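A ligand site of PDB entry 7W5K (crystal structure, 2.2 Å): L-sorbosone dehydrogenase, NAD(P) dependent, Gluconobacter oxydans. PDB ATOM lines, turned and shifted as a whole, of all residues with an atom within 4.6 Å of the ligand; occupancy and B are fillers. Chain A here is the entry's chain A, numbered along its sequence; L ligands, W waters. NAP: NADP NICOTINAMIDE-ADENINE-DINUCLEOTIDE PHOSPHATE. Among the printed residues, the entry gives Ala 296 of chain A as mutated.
O4D of the ligand sits close to O of Gly 239.
O7N of the ligand sits close to O of Glu 262.
The backbone carbonyl oxygen of Leu 263 sits close to an oxygen (O7N) of the ligand (2.8 Å).
Residues that only touch the ligand: Ile 159 (3.2 Å), Pro 161 (3.3 Å), Asn 163 (3.1 Å), Ile 168 (3.5 Å), Arg 172 (3.7 Å), Pro 187 (3.8 Å), Ala 188 (3.2 Å), Thr 218 (3.3 Å), Gly 223 (3.2 Å), Thr 227 (3.7 Å), Phe 237 (3.0 Å), Thr 238 (3.2 Å), Val 243 (3.3 Å), Gly 264 (3.0 Å), Gly 265 (3.8 Å), Ala 296 (3.2 Å), Phe 396 (3.2 Å) and Leu 422 (3.3 Å).
Hydrophobic or aromatic side chains within 4 Å of the ligand: Ile 159, Pro 161, Trp 162, Ile 168, Ala 188, Phe 237, Val 243, Ala 296, Phe 396 and Leu 422.
The nearest printed residue that does not touch the ligand is Ser 246 (4.1 Å).
The side-chain hydroxyl (OG) of Ser 240 sits at hydrogen-bond distance from the backbone NH (N) of Val 243 (3.2 Å).
O of Thr 160 is in hydrogen-bond range of N of Ala 188 (3.3 Å).
The side-chain amino group of Lys 186 lies within hydrogen-bond range of the backbone carbonyl oxygen of Gly 217, 3.2 Å away.
The backbone carbonyl oxygen (O) of Glu 262 sits at hydrogen-bond distance from the backbone NH (N) of Gly 239.
N of Glu 262 is in hydrogen-bond range of O of Phe 237.
The backbone carbonyl oxygen (O) of Thr 218 lies within hydrogen-bond range of the backbone NH (N) of Gly 223 (3.1 Å).
The guanidinium group (NH2) of Arg 172 sits at hydrogen-bond distance from the side-chain hydroxyl (OG1) of Thr 238 (2.6 Å).
The backbone carbonyl oxygen (O) of Val 243 sits at hydrogen-bond distance from the side-chain sulfur (SG) of Cys 247, 3.4 Å away.
An oxygen (O3D) of the ligand sits at hydrogen-bond distance from the side-chain carboxylate of Glu 394 (2.6 Å).
N of Glu 189 lies within hydrogen-bond range of O2X of the ligand (2.6 Å).
The backbone NH of Ser 240 lies within hydrogen-bond range of an oxygen (O2A) of the ligand (2.7 Å).
An oxygen (O2A) of the ligand is in hydrogen-bond range of the side-chain hydroxyl (OG) of Ser 240, 2.6 Å away.
O of Thr 160 is in hydrogen-bond range of O3B of the ligand (2.6 Å).
N of Gly 219 sits at hydrogen-bond distance from O3X of the ligand (2.7 Å).
NZ of Lys 186 is in salt-bridge range of O2X of the ligand (3.4 Å).
The backbone NH (N) of Gln 224 lies within hydrogen-bond range of a nitrogen (N1A) of the ligand.
OE1 of Gln 224 is in hydrogen-bond range of N6A of the ligand (2.9 Å).
The indole nitrogen (NE1) of Trp 162 lies within hydrogen-bond range of an oxygen (O1N) of the ligand (3.3 Å).
Water W3 lies within hydrogen-bond range of an oxygen (O3X) of the ligand (2.5 Å), the backbone NH of Gly 219 (3.2 Å) and the backbone NH of Arg 220 (3.3 Å).
Water W4 bridges O1X of the ligand (2.7 Å) and NE1 of Trp 162 (3.0 Å).
Water W8 lies within hydrogen-bond range of an oxygen (O2X) of the ligand and the backbone NH of Glu 189.
Water W5 lies within hydrogen-bond range of an oxygen (O5D) of the ligand, the backbone NH of Asn 163 and the backbone NH of Trp 162.
Water W7 lies within hydrogen-bond range of O3D of the ligand, N of Thr 241 and OE1 of Glu 394.
Water W9 lies within hydrogen-bond range of the backbone NH of Ala 296 and the side-chain amide nitrogen of Asn 163.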
ATOM      1  N   ILE A 159      30.002 -29.237  15.176  1.00  0.00           N
ATOM      2  CA  ILE A 159      30.217 -27.861  15.595  1.00  0.00           C
ATOM      3  C   ILE A 159      28.836 -27.259  15.813  1.00  0.00           C
ATOM      4  O   ILE A 159      27.935 -27.449  14.994  1.00  0.00           O
ATOM      5  CB  ILE A 159      31.050 -27.075  14.574  1.00  0.00           C
ATOM      6  CG1 ILE A 159      32.479 -27.686  14.513  1.00  0.00           C
ATOM      7  CG2 ILE A 159      31.077 -25.569  14.913  1.00  0.00           C
ATOM      8  CD1 ILE A 159      33.407 -27.141  13.412  1.00  0.00           C
ATOM      9  N   THR A 160      28.654 -26.643  16.967  1.00  0.00           N
ATOM     10  CA  THR A 160      27.350 -26.153  17.355  1.00  0.00           C
ATOM     11  C   THR A 160      27.473 -24.690  17.740  1.00  0.00           C
ATOM     12  O   THR A 160      28.573 -24.203  18.013  1.00  0.00           O
ATOM     13  CB  THR A 160      26.769 -26.986  18.500  1.00  0.00           C
ATOM     14  OG1 THR A 160      27.739 -27.093  19.548  1.00  0.00           O
ATOM     15  CG2 THR A 160      26.380 -28.391  17.984  1.00  0.00           C
ATOM     16  N   PRO A 161      26.372 -23.955  17.700  1.00  0.00           N
ATOM     17  CA  PRO A 161      26.411 -22.533  18.016  1.00  0.00           C
ATOM     18  C   PRO A 161      26.025 -22.272  19.461  1.00  0.00           C
ATOM     19  O   PRO A 161      25.703 -23.199  20.213  1.00  0.00           O
ATOM     20  CB  PRO A 161      25.380 -21.944  17.053  1.00  0.00           C
ATOM     21  CG  PRO A 161      24.343 -23.019  17.032  1.00  0.00           C
ATOM     22  CD  PRO A 161      25.038 -24.351  17.191  1.00  0.00           C
ATOM     23  N   TRP A 162      25.998 -20.996  19.845  1.00  0.00           N
ATOM     24  CA  TRP A 162      25.708 -20.681  21.230  1.00  0.00           C
ATOM     25  C   TRP A 162      24.232 -20.429  21.503  1.00  0.00           C
ATOM     26  O   TRP A 162      23.864 -20.219  22.660  1.00  0.00           O
ATOM     27  CB  TRP A 162      26.517 -19.460  21.667  1.00  0.00           C
ATOM     28  CG  TRP A 162      26.519 -18.333  20.717  1.00  0.00           C
ATOM     29  CD1 TRP A 162      27.571 -17.918  19.958  1.00  0.00           C
ATOM     30  CD2 TRP A 162      25.433 -17.434  20.424  1.00  0.00           C
ATOM     31  NE1 TRP A 162      27.205 -16.836  19.199  1.00  0.00           N
ATOM     32  CE2 TRP A 162      25.898 -16.511  19.467  1.00  0.00           C
ATOM     33  CE3 TRP A 162      24.115 -17.338  20.865  1.00  0.00           C
ATOM     34  CZ2 TRP A 162      25.095 -15.497  18.960  1.00  0.00           C
ATOM     35  CZ3 TRP A 162      23.317 -16.326  20.370  1.00  0.00           C
ATOM     36  CH2 TRP A 162      23.810 -15.415  19.423  1.00  0.00           C
ATOM     37  N   ASN A 163      23.376 -20.424  20.476  1.00  0.00           N
ATOM     38  CA  ASN A 163      22.008 -19.981  20.755  1.00  0.00           C
ATOM     39  C   ASN A 163      21.169 -21.070  21.400  1.00  0.00           C
ATOM     40  O   ASN A 163      20.391 -20.794  22.313  1.00  0.00           O
ATOM     41  CB  ASN A 163      21.347 -19.459  19.477  1.00  0.00           C
ATOM     42  CG  ASN A 163      21.072 -20.556  18.479  1.00  0.00           C
ATOM     43  OD1 ASN A 163      21.824 -21.531  18.406  1.00  0.00           O
ATOM     44  ND2 ASN A 163      19.998 -20.400  17.709  1.00  0.00           N
ATOM     45  N   ILE A 168      20.622 -27.903  20.321  1.00  0.00           N
ATOM     46  CA  ILE A 168      21.127 -28.221  18.987  1.00  0.00           C
ATOM     47  C   ILE A 168      22.082 -29.394  19.064  1.00  0.00           C
ATOM     48  O   ILE A 168      22.053 -30.299  18.235  1.00  0.00           O
ATOM     49  CB  ILE A 168      21.762 -26.988  18.334  1.00  0.00           C
ATOM     50  CG1 ILE A 168      20.657 -26.042  17.868  1.00  0.00           C
ATOM     51  CG2 ILE A 168      22.671 -27.436  17.185  1.00  0.00           C
ATOM     52  CD1 ILE A 168      21.124 -24.612  17.657  1.00  0.00           C
ATOM     53  N   ARG A 172      21.603 -33.269  17.247  1.00  0.00           N
ATOM     54  CA  ARG A 172      22.629 -33.739  16.339  1.00  0.00           C
ATOM     55  C   ARG A 172      23.281 -35.004  16.877  1.00  0.00           C
ATOM     56  O   ARG A 172      23.168 -36.069  16.278  1.00  0.00           O
ATOM     57  CB  ARG A 172      23.712 -32.677  16.135  1.00  0.00           C
ATOM     58  CG  ARG A 172      23.207 -31.355  15.609  1.00  0.00           C
ATOM     59  CD  ARG A 172      22.780 -31.440  14.129  1.00  0.00           C
ATOM     60  NE  ARG A 172      22.476 -30.108  13.645  1.00  0.00           N
ATOM     61  CZ  ARG A 172      21.379 -29.438  13.978  1.00  0.00           C
ATOM     62  NH1 ARG A 172      20.393 -30.022  14.639  1.00  0.00           N
ATOM     63  NH2 ARG A 172      21.284 -28.144  13.676  1.00  0.00           N
ATOM     64  N   LYS A 186      32.813 -29.599  18.938  1.00  0.00           N
ATOM     65  CA  LYS A 186      33.234 -28.291  19.452  1.00  0.00           C
ATOM     66  C   LYS A 186      31.998 -27.435  19.626  1.00  0.00           C
ATOM     67  O   LYS A 186      31.442 -26.936  18.634  1.00  0.00           O
ATOM     68  CB  LYS A 186      34.228 -27.582  18.535  1.00  0.00           C
ATOM     69  CG  LYS A 186      34.758 -26.290  19.161  1.00  0.00           C
ATOM     70  CD  LYS A 186      35.216 -25.268  18.119  1.00  0.00           C
ATOM     71  CE  LYS A 186      34.033 -24.512  17.571  1.00  0.00           C
ATOM     72  NZ  LYS A 186      33.337 -23.746  18.639  1.00  0.00           N
ATOM     73  N   PRO A 187      31.536 -27.218  20.859  1.00  0.00           N
ATOM     74  CA  PRO A 187      30.435 -26.293  21.083  1.00  0.00           C
ATOM     75  C   PRO A 187      30.937 -24.859  20.943  1.00  0.00           C
ATOM     76  O   PRO A 187      32.138 -24.602  20.815  1.00  0.00           O
ATOM     77  CB  PRO A 187      30.011 -26.592  22.517  1.00  0.00           C
ATOM     78  CG  PRO A 187      31.305 -26.959  23.162  1.00  0.00           C
ATOM     79  CD  PRO A 187      32.152 -27.648  22.129  1.00  0.00           C
ATOM     80  N   ALA A 188      29.993 -23.921  20.965  1.00  0.00           N
ATOM     81  CA  ALA A 188      30.390 -22.527  20.945  1.00  0.00           C
ATOM     82  C   ALA A 188      31.298 -22.254  22.130  1.00  0.00           C
ATOM     83  O   ALA A 188      31.090 -22.798  23.219  1.00  0.00           O
ATOM     84  CB  ALA A 188      29.182 -21.604  20.976  1.00  0.00           C
ATOM     85  N   GLU A 189      32.345 -21.487  21.891  1.00  0.00           N
ATOM     86  CA  GLU A 189      33.239 -21.113  22.977  1.00  0.00           C
ATOM     87  C   GLU A 189      32.472 -20.560  24.168  1.00  0.00           C
ATOM     88  O   GLU A 189      32.790 -20.877  25.320  1.00  0.00           O
ATOM     89  CB  GLU A 189      34.242 -20.089  22.476  1.00  0.00           C
ATOM     90  CG  GLU A 189      35.303 -19.759  23.481  1.00  0.00           C
ATOM     91  CD  GLU A 189      36.184 -18.618  23.019  1.00  0.00           C
ATOM     92  OE1 GLU A 189      35.672 -17.657  22.405  1.00  0.00           O
ATOM     93  OE2 GLU A 189      37.410 -18.684  23.286  1.00  0.00           O
ATOM     94  N   GLY A 217      36.897 -24.748  22.440  1.00  0.00           N
ATOM     95  CA  GLY A 217      37.772 -23.740  21.886  1.00  0.00           C
ATOM     96  C   GLY A 217      37.052 -22.969  20.813  1.00  0.00           C
ATOM     97  O   GLY A 217      35.860 -23.157  20.578  1.00  0.00           O
ATOM     98  N   THR A 218      37.797 -22.129  20.126  1.00  0.00           N
ATOM     99  CA  THR A 218      37.186 -21.214  19.184  1.00  0.00           C
ATOM    100  C   THR A 218      36.985 -21.905  17.850  1.00  0.00           C
ATOM    101  O   THR A 218      37.717 -22.833  17.480  1.00  0.00           O
ATOM    102  CB  THR A 218      38.047 -19.974  19.008  1.00  0.00           C
ATOM    103  OG1 THR A 218      39.268 -20.344  18.367  1.00  0.00           O
ATOM    104  CG2 THR A 218      38.350 -19.374  20.355  1.00  0.00           C
ATOM    105  N   GLY A 219      35.967 -21.443  17.123  1.00  0.00           N
ATOM    106  CA  GLY A 219      35.754 -21.944  15.771  1.00  0.00           C
ATOM    107  C   GLY A 219      36.940 -21.671  14.864  1.00  0.00           C
ATOM    108  O   GLY A 219      37.221 -22.457  13.957  1.00  0.00           O
ATOM    109  N   ARG A 220      37.676 -20.541  15.215  1.00  0.00           N
ATOM    110  CA  ARG A 220      38.806 -20.168  14.329  1.00  0.00           C
ATOM    111  C   ARG A 220      40.007 -21.073  14.617  1.00  0.00           C
ATOM    112  O   ARG A 220      40.856 -21.204  13.728  1.00  0.00           O
ATOM    113  CB  ARG A 220      39.126 -18.669  14.404  1.00  0.00           C
ATOM    114  CG  ARG A 220      38.089 -17.783  13.729  1.00  0.00           C
ATOM    115  CD  ARG A 220      38.681 -16.653  12.919  1.00  0.00           C
ATOM    116  NE  ARG A 220      39.821 -16.012  13.560  1.00  0.00           N
ATOM    117  CZ  ARG A 220      39.749 -15.264  14.649  1.00  0.00           C
ATOM    118  NH1 ARG A 220      38.589 -15.059  15.234  1.00  0.00           N
ATOM    119  NH2 ARG A 220      40.843 -14.729  15.157  1.00  0.00           N
ATOM    120  N   GLY A 223      37.530 -25.307  15.637  1.00  0.00           N
ATOM    121  CA  GLY A 223      36.532 -25.514  14.611  1.00  0.00           C
ATOM    122  C   GLY A 223      37.141 -25.585  13.221  1.00  0.00           C
ATOM    123  O   GLY A 223      36.842 -26.495  12.451  1.00  0.00           O
ATOM    124  N   GLN A 224      37.986 -24.603  12.880  1.00  0.00           N
ATOM    125  CA  GLN A 224      38.620 -24.609  11.573  1.00  0.00           C
ATOM    126  C   GLN A 224      39.450 -25.867  11.384  1.00  0.00           C
ATOM    127  O   GLN A 224      39.475 -26.441  10.290  1.00  0.00           O
ATOM    128  CB  GLN A 224      39.496 -23.373  11.389  1.00  0.00           C
ATOM    129  CG  GLN A 224      40.179 -23.338  10.009  1.00  0.00           C
ATOM    130  CD  GLN A 224      39.182 -23.076   8.890  1.00  0.00           C
ATOM    131  OE1 GLN A 224      38.206 -22.349   9.073  1.00  0.00           O
ATOM    132  NE2 GLN A 224      39.408 -23.682   7.726  1.00  0.00           N
ATOM    133  N   THR A 227      37.022 -28.675  10.549  1.00  0.00           N
ATOM    134  CA  THR A 227      36.546 -28.666   9.173  1.00  0.00           C
ATOM    135  C   THR A 227      37.652 -29.074   8.221  1.00  0.00           C
ATOM    136  O   THR A 227      37.395 -29.661   7.166  1.00  0.00           O
ATOM    137  CB  THR A 227      36.007 -27.292   8.808  1.00  0.00           C
ATOM    138  OG1 THR A 227      37.043 -26.319   8.926  1.00  0.00           O
ATOM    139  CG2 THR A 227      34.842 -26.941   9.725  1.00  0.00           C
ATOM    140  N   PHE A 237      27.731 -29.105  11.035  1.00  0.00           N
ATOM    141  CA  PHE A 237      27.959 -27.716  11.403  1.00  0.00           C
ATOM    142  C   PHE A 237      26.635 -27.002  11.515  1.00  0.00           C
ATOM    143  O   PHE A 237      25.826 -27.001  10.576  1.00  0.00           O
ATOM    144  CB  PHE A 237      28.846 -26.978  10.413  1.00  0.00           C
ATOM    145  CG  PHE A 237      28.950 -25.535  10.727  1.00  0.00           C
ATOM    146  CD1 PHE A 237      29.781 -25.110  11.722  1.00  0.00           C
ATOM    147  CD2 PHE A 237      28.122 -24.608  10.079  1.00  0.00           C
ATOM    148  CE1 PHE A 237      29.836 -23.776  12.052  1.00  0.00           C
ATOM    149  CE2 PHE A 237      28.178 -23.278  10.400  1.00  0.00           C
ATOM    150  CZ  PHE A 237      29.044 -22.859  11.403  1.00  0.00           C
ATOM    151  N   THR A 238      26.419 -26.343  12.642  1.00  0.00           N
ATOM    152  CA  THR A 238      25.254 -25.502  12.822  1.00  0.00           C
ATOM    153  C   THR A 238      25.756 -24.128  13.221  1.00  0.00           C
ATOM    154  O   THR A 238      26.467 -23.996  14.227  1.00  0.00           O
ATOM    155  CB  THR A 238      24.306 -26.080  13.858  1.00  0.00           C
ATOM    156  OG1 THR A 238      23.787 -27.328  13.381  1.00  0.00           O
ATOM    157  CG2 THR A 238      23.169 -25.167  14.027  1.00  0.00           C
ATOM    158  N   GLY A 239      25.418 -23.133  12.432  1.00  0.00           N
ATOM    159  CA  GLY A 239      25.949 -21.800  12.641  1.00  0.00           C
ATOM    160  C   GLY A 239      25.695 -20.977  11.396  1.00  0.00           C
ATOM    161  O   GLY A 239      24.811 -21.285  10.594  1.00  0.00           O
ATOM    162  N   SER A 240      26.463 -19.906  11.272  1.00  0.00           N
ATOM    163  CA  SER A 240      26.183 -18.949  10.226  1.00  0.00           C
ATOM    164  C   SER A 240      26.481 -19.532   8.844  1.00  0.00           C
ATOM    165  O   SER A 240      27.318 -20.433   8.687  1.00  0.00           O
ATOM    166  CB  SER A 240      27.000 -17.679  10.447  1.00  0.00           C
ATOM    167  OG  SER A 240      28.359 -18.022  10.489  1.00  0.00           O
ATOM    168  N   THR A 241      25.755 -19.030   7.850  1.00  0.00           N
ATOM    169  CA  THR A 241      26.073 -19.387   6.479  1.00  0.00           C
ATOM    170  C   THR A 241      27.505 -18.985   6.148  1.00  0.00           C
ATOM    171  O   THR A 241      28.210 -19.728   5.453  1.00  0.00           O
ATOM    172  CB  THR A 241      25.064 -18.720   5.546  1.00  0.00           C
ATOM    173  OG1 THR A 241      23.758 -19.109   5.954  1.00  0.00           O
ATOM    174  CG2 THR A 241      25.271 -19.165   4.105  1.00  0.00           C
ATOM    175  N   VAL A 243      30.211 -19.019   8.101  1.00  0.00           N
ATOM    176  CA  VAL A 243      31.119 -20.057   8.566  1.00  0.00           C
ATOM    177  C   VAL A 243      30.795 -21.378   7.891  1.00  0.00           C
ATOM    178  O   VAL A 243      31.693 -22.181   7.601  1.00  0.00           O
ATOM    179  CB  VAL A 243      31.077 -20.159  10.094  1.00  0.00           C
ATOM    180  CG1 VAL A 243      31.872 -21.369  10.543  1.00  0.00           C
ATOM    181  CG2 VAL A 243      31.628 -18.877  10.717  1.00  0.00           C
ATOM    182  N   SER A 246      32.894 -21.499   5.130  1.00  0.00           N
ATOM    183  CA  SER A 246      34.251 -21.875   5.528  1.00  0.00           C
ATOM    184  C   SER A 246      34.378 -23.388   5.664  1.00  0.00           C
ATOM    185  O   SER A 246      35.352 -23.975   5.194  1.00  0.00           O
ATOM    186  CB  SER A 246      34.626 -21.214   6.842  1.00  0.00           C
ATOM    187  OG  SER A 246      35.054 -19.879   6.630  1.00  0.00           O
ATOM    188  N   CYS A 247      33.373 -24.036   6.264  1.00  0.00           N
ATOM    189  CA  CYS A 247      33.371 -25.493   6.333  1.00  0.00           C
ATOM    190  C   CYS A 247      33.450 -26.128   4.949  1.00  0.00           C
ATOM    191  O   CYS A 247      34.209 -27.071   4.737  1.00  0.00           O
ATOM    192  CB  CYS A 247      32.107 -25.987   7.037  1.00  0.00           C
ATOM    193  SG  CYS A 247      31.881 -25.358   8.665  1.00  0.00           S
ATOM    194  N   GLU A 262      23.657 -26.569   8.928  1.00  0.00           N
ATOM    195  CA  GLU A 262      22.457 -25.947   9.441  1.00  0.00           C
ATOM    196  C   GLU A 262      22.852 -24.493   9.617  1.00  0.00           C
ATOM    197  O   GLU A 262      23.532 -24.142  10.586  1.00  0.00           O
ATOM    198  CB  GLU A 262      21.995 -26.596  10.733  1.00  0.00           C
ATOM    199  CG  GLU A 262      21.521 -28.020  10.488  1.00  0.00           C
ATOM    200  CD  GLU A 262      20.290 -28.063   9.586  1.00  0.00           C
ATOM    201  OE1 GLU A 262      19.419 -27.187   9.739  1.00  0.00           O
ATOM    202  OE2 GLU A 262      20.185 -28.969   8.737  1.00  0.00           O
ATOM    203  N   LEU A 263      22.461 -23.675   8.651  1.00  0.00           N
ATOM    204  CA  LEU A 263      23.060 -22.377   8.514  1.00  0.00           C
ATOM    205  C   LEU A 263      22.047 -21.299   8.919  1.00  0.00           C
ATOM    206  O   LEU A 263      21.153 -21.566   9.757  1.00  0.00           O
ATOM    207  CB  LEU A 263      23.593 -22.234   7.105  1.00  0.00           C
ATOM    208  CG  LEU A 263      24.534 -23.399   6.792  1.00  0.00           C
ATOM    209  CD1 LEU A 263      25.133 -23.210   5.414  1.00  0.00           C
ATOM    210  CD2 LEU A 263      25.610 -23.497   7.848  1.00  0.00           C
ATOM    211  N   GLY A 264      22.190 -20.116   8.364  1.00  0.00           N
ATOM    212  CA  GLY A 264      21.359 -19.005   8.731  1.00  0.00           C
ATOM    213  C   GLY A 264      19.961 -19.130   8.144  1.00  0.00           C
ATOM    214  O   GLY A 264      19.625 -20.050   7.397  1.00  0.00           O
ATOM    215  N   GLY A 265      19.151 -18.143   8.486  1.00  0.00           N
ATOM    216  CA  GLY A 265      17.813 -18.055   7.944  1.00  0.00           C
ATOM    217  C   GLY A 265      17.356 -16.627   8.048  1.00  0.00           C
ATOM    218  O   GLY A 265      17.917 -15.817   8.789  1.00  0.00           O
ATOM    219  N   ALA A 296      17.695 -19.515  14.546  1.00  0.00           N
ATOM    220  CA  ALA A 296      17.798 -19.544  13.092  1.00  0.00           C
ATOM    221  C   ALA A 296      16.454 -19.772  12.429  1.00  0.00           C
ATOM    222  O   ALA A 296      16.293 -19.421  11.257  1.00  0.00           O
ATOM    223  CB  ALA A 296      18.750 -20.657  12.663  1.00  0.00           C
ATOM    224  N   GLN A 343      26.969 -10.306  19.136  1.00  0.00           N
ATOM    225  CA  GLN A 343      25.605 -10.423  18.628  1.00  0.00           C
ATOM    226  C   GLN A 343      24.750  -9.280  19.134  1.00  0.00           C
ATOM    227  O   GLN A 343      23.895  -8.769  18.402  1.00  0.00           O
ATOM    228  CB  GLN A 343      24.961 -11.755  18.992  1.00  0.00           C
ATOM    229  CG  GLN A 343      23.744 -12.067  18.106  1.00  0.00           C
ATOM    230  CD  GLN A 343      24.096 -11.998  16.622  1.00  0.00           C
ATOM    231  OE1 GLN A 343      23.480 -11.259  15.849  1.00  0.00           O
ATOM    232  NE2 GLN A 343      25.105 -12.767  16.217  1.00  0.00           N
ATOM    233  N   GLU A 394      20.219 -11.638   8.215  1.00  0.00           N
ATOM    234  CA  GLU A 394      19.778 -12.254   9.448  1.00  0.00           C
ATOM    235  C   GLU A 394      20.292 -11.419  10.611  1.00  0.00           C
ATOM    236  O   GLU A 394      21.506 -11.245  10.788  1.00  0.00           O
ATOM    237  CB  GLU A 394      20.291 -13.685   9.545  1.00  0.00           C
ATOM    238  CG  GLU A 394      19.957 -14.304  10.838  1.00  0.00           C
ATOM    239  CD  GLU A 394      20.184 -15.793  10.838  1.00  0.00           C
ATOM    240  OE1 GLU A 394      21.120 -16.235  10.153  1.00  0.00           O
ATOM    241  OE2 GLU A 394      19.446 -16.508  11.552  1.00  0.00           O
ATOM    242  N   PHE A 396      19.482 -12.103  13.811  1.00  0.00           N
ATOM    243  CA  PHE A 396      19.704 -13.033  14.926  1.00  0.00           C
ATOM    244  C   PHE A 396      19.429 -12.341  16.255  1.00  0.00           C
ATOM    245  O   PHE A 396      20.182 -12.470  17.219  1.00  0.00           O
ATOM    246  CB  PHE A 396      21.106 -13.645  14.908  1.00  0.00           C
ATOM    247  CG  PHE A 396      21.123 -15.065  15.377  1.00  0.00           C
ATOM    248  CD1 PHE A 396      20.388 -16.023  14.712  1.00  0.00           C
ATOM    249  CD2 PHE A 396      21.860 -15.439  16.499  1.00  0.00           C
ATOM    250  CE1 PHE A 396      20.368 -17.336  15.157  1.00  0.00           C
ATOM    251  CE2 PHE A 396      21.871 -16.748  16.922  1.00  0.00           C
ATOM    252  CZ  PHE A 396      21.113 -17.695  16.260  1.00  0.00           C
ATOM    253  N   LEU A 422      15.544 -21.705   5.447  1.00  0.00           N
ATOM    254  CA  LEU A 422      15.542 -22.613   6.579  1.00  0.00           C
ATOM    255  C   LEU A 422      14.125 -22.947   7.013  1.00  0.00           C
ATOM    256  O   LEU A 422      13.772 -24.116   7.149  1.00  0.00           O
ATOM    257  CB  LEU A 422      16.313 -21.999   7.741  1.00  0.00           C
ATOM    258  CG  LEU A 422      16.504 -22.983   8.902  1.00  0.00           C
ATOM    259  CD1 LEU A 422      17.080 -24.313   8.390  1.00  0.00           C
ATOM    260  CD2 LEU A 422      17.377 -22.388   9.985  1.00  0.00           C
HETATM  261  PA  NAP L   1      28.914 -18.917  13.821  1.00  0.00           P
HETATM  262  O1A NAP L   1      29.698 -17.660  13.954  1.00  0.00           O
HETATM  263  O2A NAP L   1      28.895 -19.602  12.507  1.00  0.00           O
HETATM  264  O5B NAP L   1      29.380 -19.941  14.947  1.00  0.00           O
HETATM  265  C5B NAP L   1      28.815 -21.282  14.986  1.00  0.00           C
HETATM  266  C4B NAP L   1      29.858 -22.237  15.494  1.00  0.00           C
HETATM  267  O4B NAP L   1      30.891 -22.383  14.490  1.00  0.00           O
HETATM  268  C3B NAP L   1      30.587 -21.835  16.783  1.00  0.00           C
HETATM  269  O3B NAP L   1      30.850 -22.975  17.580  1.00  0.00           O
HETATM  270  C2B NAP L   1      31.871 -21.212  16.240  1.00  0.00           C
HETATM  271  O2B NAP L   1      32.954 -21.248  17.153  1.00  0.00           O
HETATM  272  C1B NAP L   1      32.142 -22.156  15.085  1.00  0.00           C
HETATM  273  N9A NAP L   1      33.058 -21.633  14.096  1.00  0.00           N
HETATM  274  C8A NAP L   1      33.387 -20.314  13.880  1.00  0.00           C
HETATM  275  N7A NAP L   1      34.248 -20.148  12.919  1.00  0.00           N
HETATM  276  C5A NAP L   1      34.512 -21.437  12.459  1.00  0.00           C
HETATM  277  C6A NAP L   1      35.343 -21.918  11.443  1.00  0.00           C
HETATM  278  N6A NAP L   1      36.105 -21.142  10.678  1.00  0.00           N
HETATM  279  N1A NAP L   1      35.379 -23.255  11.251  1.00  0.00           N
HETATM  280  C2A NAP L   1      34.616 -24.026  12.024  1.00  0.00           C
HETATM  281  N3A NAP L   1      33.792 -23.686  13.013  1.00  0.00           N
HETATM  282  C4A NAP L   1      33.780 -22.356  13.178  1.00  0.00           C
HETATM  283  O3  NAP L   1      27.403 -18.622  14.271  1.00  0.00           O
HETATM  284  PN  NAP L   1      26.787 -18.100  15.656  1.00  0.00           P
HETATM  285  O1N NAP L   1      27.176 -19.040  16.741  1.00  0.00           O
HETATM  286  O2N NAP L   1      27.150 -16.667  15.804  1.00  0.00           O
HETATM  287  O5D NAP L   1      25.219 -18.225  15.387  1.00  0.00           O
HETATM  288  C5D NAP L   1      24.562 -17.260  14.527  1.00  0.00           C
HETATM  289  C4D NAP L   1      24.317 -17.880  13.174  1.00  0.00           C
HETATM  290  O4D NAP L   1      24.162 -19.305  13.331  1.00  0.00           O
HETATM  291  C3D NAP L   1      23.051 -17.406  12.444  1.00  0.00           C
HETATM  292  O3D NAP L   1      23.302 -17.204  11.060  1.00  0.00           O
HETATM  293  C2D NAP L   1      22.079 -18.557  12.696  1.00  0.00           C
HETATM  294  O2D NAP L   1      21.033 -18.653  11.743  1.00  0.00           O
HETATM  295  C1D NAP L   1      23.016 -19.750  12.623  1.00  0.00           C
HETATM  296  N1N NAP L   1      22.472 -20.940  13.334  1.00  0.00           N
HETATM  297  C2N NAP L   1      21.913 -21.965  12.636  1.00  0.00           C
HETATM  298  C3N NAP L   1      21.044 -22.831  13.297  1.00  0.00           C
HETATM  299  C7N NAP L   1      20.267 -23.853  12.502  1.00  0.00           C
HETATM  300  O7N NAP L   1      20.153 -23.722  11.290  1.00  0.00           O
HETATM  301  N7N NAP L   1      19.729 -24.862  13.178  1.00  0.00           N
HETATM  302  C4N NAP L   1      20.905 -22.734  14.666  1.00  0.00           C
HETATM  303  C5N NAP L   1      21.689 -21.844  15.372  1.00  0.00           C
HETATM  304  C6N NAP L   1      22.519 -20.994  14.679  1.00  0.00           C
HETATM  305  P2B NAP L   1      32.973 -20.001  18.167  1.00  0.00           P
HETATM  306  O1X NAP L   1      32.137 -18.894  17.608  1.00  0.00           O
HETATM  307  O2X NAP L   1      32.409 -20.538  19.457  1.00  0.00           O
HETATM  308  O3X NAP L   1      34.403 -19.602  18.313  1.00  0.00           O
HETATM  309  O   HOH W   1      32.163 -17.648  15.491  1.00  0.00           O
HETATM  310  O   HOH W   2      34.711 -17.454  12.434  1.00  0.00           O
HETATM  311  O   HOH W   3      35.593 -18.304  16.474  1.00  0.00           O
HETATM  312  O   HOH W   4      29.624 -17.967  17.788  1.00  0.00           O
HETATM  313  O   HOH W   5      24.243 -18.904  18.077  1.00  0.00           O
HETATM  314  O   HOH W   6      31.299 -15.779  12.344  1.00  0.00           O
HETATM  315  O   HOH W   7      23.862 -16.557   8.210  1.00  0.00           O
HETATM  316  O   HOH W   8      31.248 -18.510  20.939  1.00  0.00           O
HETATM  317  O   HOH W   9      18.088 -22.066  16.084  1.00  0.00           O
HETATM  318  O   HOH W  10      35.806 -23.701   8.650  1.00  0.00           O
